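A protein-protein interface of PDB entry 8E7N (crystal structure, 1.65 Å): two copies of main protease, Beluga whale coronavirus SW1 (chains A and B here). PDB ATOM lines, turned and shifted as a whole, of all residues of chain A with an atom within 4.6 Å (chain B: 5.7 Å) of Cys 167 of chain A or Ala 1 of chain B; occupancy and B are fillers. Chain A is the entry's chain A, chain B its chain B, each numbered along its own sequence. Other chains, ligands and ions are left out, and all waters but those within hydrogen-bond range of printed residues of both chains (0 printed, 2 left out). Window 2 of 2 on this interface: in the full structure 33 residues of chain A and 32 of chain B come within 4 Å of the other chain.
The side-chain sulfur (SG) of Cys 167 of chain A sits at hydrogen-bond distance from the side-chain amide oxygen (OD1) of Asn 211 of chain B (3.4 Å). N of Ala 1 of chain B lies within hydrogen-bond range of O of Phe 137 of chain A. The backbone carbonyl oxygen of Gly 2 of chain B is in hydrogen-bond range of the side-chain hydroxyl of Ser 136 of chain A (3.2 Å). OE1 of Gln 296 of chain B lies within hydrogen-bond range of OG of Ser 136 of chain A (2.7 Å). The backbone NH (N) of Ala 1 of chain B lies within hydrogen-bond range of the side-chain carboxylate (OE1) of Glu 163 of chain A (2.8 Å). O of Ala 1 of chain B lies close to NE2 of His 169 of chain A, at 3.3 Å.
The backbone NH (N) of Gly 2 of chain B is in hydrogen-bond range of the side-chain amide oxygen (OD1) of Asn 211 of chain B. ND1 of His 169 of chain A sits at hydrogen-bond distance from N of Gly 135 of chain A (3.0 Å). A ring nitrogen (NE2) of His 169 of chain A sits at hydrogen-bond distance from the side-chain carboxylate (OE1) of Glu 163 of chain A.
Among the printed residues, pairs that only touch across the chains: Gly 135 of chain A with Gly 2 of chain B (3.3 Å), Ser 136 of chain A with Ala 1 of chain B (3.4 Å), Cys 167 of chain A with Ala 1 of chain B (3.6 Å), Gly 135 of chain A with Ala 1 of chain B (3.8 Å) and Gly 135 of chain A with Ile 3 of chain B (3.98 Å).
Cys 167 of chain A touches just these residues of chain B: Ala 1 and Asn 211. Ala 1 of chain B touches just these residues of chain A: Gly 135, Ser 136, Phe 137, Glu 163, Cys 167 and His 169. Of the printed residues of chain A, Asn 211 of chain B touches Cys 167. Of the printed residues of chain A, Gly 2 of chain B touches Gly 135 (3.3 Å) and Ser 136 (3.2 Å). Of the printed residues of chain B, Ser 136 of chain A touches Ala 1, Gly 2 and Gln 296. Gly 166 of chain A touches none of the printed residues of chain B. The nearest residue of chain B that does not touch Cys 167 of chain A is Gly 2 of chain B (4.2 Å).
Of the 6 printed residues of chain B, 5 touch a printed residue of chain A. Hydrophobic or aromatic side chains of chain B that line the printed part of chain A: Ala 1. Of the 10 printed residues of chain A, 6 touch a printed residue of chain B. Among the printed residues, no Asp or Glu carboxylate lies within 4 Å of a Lys or Arg side-chain nitrogen of the other chain.
No position is printed for both chains.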
ATOM      1  N   GLY A 135     -15.018  -8.258 -29.369  1.00  0.00           N
ATOM      2  CA  GLY A 135     -16.241  -7.512 -29.453  1.00  0.00           C
ATOM      3  C   GLY A 135     -16.673  -7.046 -28.089  1.00  0.00           C
ATOM      4  O   GLY A 135     -15.861  -6.948 -27.151  1.00  0.00           O
ATOM      5  N   SER A 136     -17.995  -6.823 -27.955  1.00  0.00           N
ATOM      6  CA  SER A 136     -18.593  -6.379 -26.698  1.00  0.00           C
ATOM      7  C   SER A 136     -20.006  -6.938 -26.715  1.00  0.00           C
ATOM      8  O   SER A 136     -20.876  -6.417 -27.432  1.00  0.00           O
ATOM      9  CB  SER A 136     -18.595  -4.856 -26.559  1.00  0.00           C
ATOM     10  OG  SER A 136     -19.370  -4.450 -25.463  1.00  0.00           O
ATOM     11  N   PHE A 137     -20.213  -7.997 -25.927  1.00  0.00           N
ATOM     12  CA  PHE A 137     -21.489  -8.687 -25.989  1.00  0.00           C
ATOM     13  C   PHE A 137     -21.839  -9.159 -24.580  1.00  0.00           C
ATOM     14  O   PHE A 137     -20.962  -9.634 -23.874  1.00  0.00           O
ATOM     15  CB  PHE A 137     -21.390  -9.929 -26.860  1.00  0.00           C
ATOM     16  CG  PHE A 137     -21.206  -9.667 -28.337  1.00  0.00           C
ATOM     17  CD1 PHE A 137     -22.311  -9.241 -29.110  1.00  0.00           C
ATOM     18  CD2 PHE A 137     -19.992  -9.947 -28.948  1.00  0.00           C
ATOM     19  CE1 PHE A 137     -22.152  -9.104 -30.536  1.00  0.00           C
ATOM     20  CE2 PHE A 137     -19.799  -9.808 -30.368  1.00  0.00           C
ATOM     21  CZ  PHE A 137     -20.875  -9.369 -31.151  1.00  0.00           C
ATOM     22  N   GLU A 163     -18.935 -16.348 -26.024  1.00  0.00           N
ATOM     23  CA  GLU A 163     -17.768 -15.642 -25.501  1.00  0.00           C
ATOM     24  C   GLU A 163     -16.755 -16.655 -24.995  1.00  0.00           C
ATOM     25  O   GLU A 163     -17.107 -17.578 -24.245  1.00  0.00           O
ATOM     26  CB  GLU A 163     -18.187 -14.728 -24.380  1.00  0.00           C
ATOM     27  CG  GLU A 163     -17.071 -13.824 -23.825  1.00  0.00           C
ATOM     28  CD  GLU A 163     -17.718 -12.803 -22.957  1.00  0.00           C
ATOM     29  OE1 GLU A 163     -18.212 -11.788 -23.462  1.00  0.00           O
ATOM     30  OE2 GLU A 163     -17.897 -13.069 -21.738  1.00  0.00           O
ATOM     31  N   LEU A 164     -15.548 -16.511 -25.434  1.00  0.00           N
ATOM     32  CA  LEU A 164     -14.435 -17.378 -25.117  1.00  0.00           C
ATOM     33  C   LEU A 164     -13.561 -16.735 -24.081  1.00  0.00           C
ATOM     34  O   LEU A 164     -13.705 -15.547 -23.766  1.00  0.00           O
ATOM     35  CB  LEU A 164     -13.598 -17.626 -26.352  1.00  0.00           C
ATOM     36  CG  LEU A 164     -14.311 -18.527 -27.359  1.00  0.00           C
ATOM     37  CD1 LEU A 164     -13.803 -18.105 -28.742  1.00  0.00           C
ATOM     38  CD2 LEU A 164     -14.091 -20.027 -27.072  1.00  0.00           C
ATOM     39  N   PRO A 165     -12.625 -17.504 -23.513  1.00  0.00           N
ATOM     40  CA  PRO A 165     -11.805 -16.946 -22.438  1.00  0.00           C
ATOM     41  C   PRO A 165     -11.030 -15.742 -22.953  1.00  0.00           C
ATOM     42  O   PRO A 165     -10.578 -15.697 -24.100  1.00  0.00           O
ATOM     43  CB  PRO A 165     -10.851 -18.100 -22.060  1.00  0.00           C
ATOM     44  CG  PRO A 165     -11.580 -19.396 -22.523  1.00  0.00           C
ATOM     45  CD  PRO A 165     -12.388 -18.951 -23.746  1.00  0.00           C
ATOM     46  N   GLY A 166     -10.852 -14.765 -22.078  1.00  0.00           N
ATOM     47  CA  GLY A 166     -10.092 -13.599 -22.455  1.00  0.00           C
ATOM     48  C   GLY A 166     -10.938 -12.538 -23.091  1.00  0.00           C
ATOM     49  O   GLY A 166     -10.402 -11.677 -23.784  1.00  0.00           O
ATOM     50  N   CYS A 167     -12.248 -12.566 -22.843  1.00  0.00           N
ATOM     51  CA  CYS A 167     -13.134 -11.554 -23.379  1.00  0.00           C
ATOM     52  C   CYS A 167     -13.019 -11.547 -24.903  1.00  0.00           C
ATOM     53  O   CYS A 167     -12.924 -10.486 -25.551  1.00  0.00           O
ATOM     54  CB  CYS A 167     -12.831 -10.181 -22.748  1.00  0.00           C
ATOM     55  SG  CYS A 167     -13.129 -10.158 -20.874  1.00  0.00           S
ATOM     56  N   VAL A 168     -12.944 -12.740 -25.499  1.00  0.00           N
ATOM     57  CA  VAL A 168     -12.972 -12.802 -26.968  1.00  0.00           C
ATOM     58  C   VAL A 168     -14.231 -13.559 -27.397  1.00  0.00           C
ATOM     59  O   VAL A 168     -14.920 -14.189 -26.570  1.00  0.00           O
ATOM     60  CB  VAL A 168     -11.717 -13.393 -27.644  1.00  0.00           C
ATOM     61  CG1 VAL A 168     -10.385 -12.820 -27.060  1.00  0.00           C
ATOM     62  CG2 VAL A 168     -11.712 -14.901 -27.778  1.00  0.00           C
ATOM     63  N   HIS A 169     -14.602 -13.349 -28.676  1.00  0.00           N
ATOM     64  CA  HIS A 169     -15.931 -13.717 -29.134  1.00  0.00           C
ATOM     65  C   HIS A 169     -15.848 -14.602 -30.363  1.00  0.00           C
ATOM     66  O   HIS A 169     -14.975 -14.446 -31.222  1.00  0.00           O
ATOM     67  CB  HIS A 169     -16.790 -12.422 -29.395  1.00  0.00           C
ATOM     68  CG  HIS A 169     -16.999 -11.646 -28.125  1.00  0.00           C
ATOM     69  ND1 HIS A 169     -16.326 -10.484 -27.813  1.00  0.00           N
ATOM     70  CD2 HIS A 169     -17.734 -11.961 -27.027  1.00  0.00           C
ATOM     71  CE1 HIS A 169     -16.672 -10.083 -26.598  1.00  0.00           C
ATOM     72  NE2 HIS A 169     -17.541 -10.958 -26.098  1.00  0.00           N
ATOM     73  N   ALA B   1     -18.940  -9.545 -22.005  1.00  0.00           N
ATOM     74  CA  ALA B   1     -17.696  -8.784 -21.735  1.00  0.00           C
ATOM     75  C   ALA B   1     -17.161  -8.158 -23.000  1.00  0.00           C
ATOM     76  O   ALA B   1     -17.726  -8.349 -24.121  1.00  0.00           O
ATOM     77  CB  ALA B   1     -16.671  -9.675 -21.161  1.00  0.00           C
ATOM     78  N   GLY B   2     -16.054  -7.446 -22.845  1.00  0.00           N
ATOM     79  CA  GLY B   2     -15.487  -6.644 -23.906  1.00  0.00           C
ATOM     80  C   GLY B   2     -15.913  -5.201 -23.788  1.00  0.00           C
ATOM     81  O   GLY B   2     -16.998  -4.880 -23.316  1.00  0.00           O
ATOM     82  N   ILE B   3     -15.064  -4.315 -24.281  1.00  0.00           N
ATOM     83  CA  ILE B   3     -15.350  -2.884 -24.216  1.00  0.00           C
ATOM     84  C   ILE B   3     -15.084  -2.277 -25.579  1.00  0.00           C
ATOM     85  O   ILE B   3     -13.970  -2.378 -26.101  1.00  0.00           O
ATOM     86  CB  ILE B   3     -14.498  -2.171 -23.142  1.00  0.00           C
ATOM     87  CG1 ILE B   3     -14.874  -2.651 -21.742  1.00  0.00           C
ATOM     88  CG2 ILE B   3     -14.691  -0.619 -23.300  1.00  0.00           C
ATOM     89  CD1 ILE B   3     -16.312  -2.308 -21.332  1.00  0.00           C
ATOM     90  N   ASN B 211     -13.692  -6.433 -16.779  1.00  0.00           N
ATOM     91  CA  ASN B 211     -13.155  -7.349 -17.762  1.00  0.00           C
ATOM     92  C   ASN B 211     -11.908  -8.076 -17.285  1.00  0.00           C
ATOM     93  O   ASN B 211     -11.058  -8.456 -18.103  1.00  0.00           O
ATOM     94  CB  ASN B 211     -12.891  -6.595 -19.069  1.00  0.00           C
ATOM     95  CG  ASN B 211     -14.187  -6.316 -19.784  1.00  0.00           C
ATOM     96  OD1 ASN B 211     -14.554  -7.081 -20.656  1.00  0.00           O
ATOM     97  ND2 ASN B 211     -14.919  -5.283 -19.367  1.00  0.00           N
ATOM     98  N   ASN B 212     -11.735  -8.222 -15.956  1.00  0.00           N
ATOM     99  CA  ASN B 212     -10.638  -8.998 -15.351  1.00  0.00           C
ATOM    100  C   ASN B 212      -9.280  -8.405 -15.621  1.00  0.00           C
ATOM    101  O   ASN B 212      -8.256  -9.092 -15.521  1.00  0.00           O
ATOM    102  CB  ASN B 212     -10.631 -10.453 -15.831  1.00  0.00           C
ATOM    103  CG  ASN B 212     -11.950 -11.127 -15.627  1.00  0.00           C
ATOM    104  OD1 ASN B 212     -12.450 -11.182 -14.499  1.00  0.00           O
ATOM    105  ND2 ASN B 212     -12.545 -11.654 -16.729  1.00  0.00           N
ATOM    106  N   GLN B 296     -22.230  -1.481 -21.225  1.00  0.00           N
ATOM    107  CA  GLN B 296     -21.492  -2.674 -21.618  1.00  0.00           C
ATOM    108  C   GLN B 296     -21.091  -3.529 -20.458  1.00  0.00           C
ATOM    109  O   GLN B 296     -20.324  -4.477 -20.636  1.00  0.00           O
ATOM    110  CB  GLN B 296     -20.204  -2.267 -22.355  1.00  0.00           C
ATOM    111  CG  GLN B 296     -20.537  -1.524 -23.572  1.00  0.00           C
ATOM    112  CD  GLN B 296     -19.251  -1.136 -24.286  1.00  0.00           C
ATOM    113  OE1 GLN B 296     -18.572  -1.991 -24.844  1.00  0.00           O
ATOM    114  NE2 GLN B 296     -18.899   0.157 -24.242  1.00  0.00           N
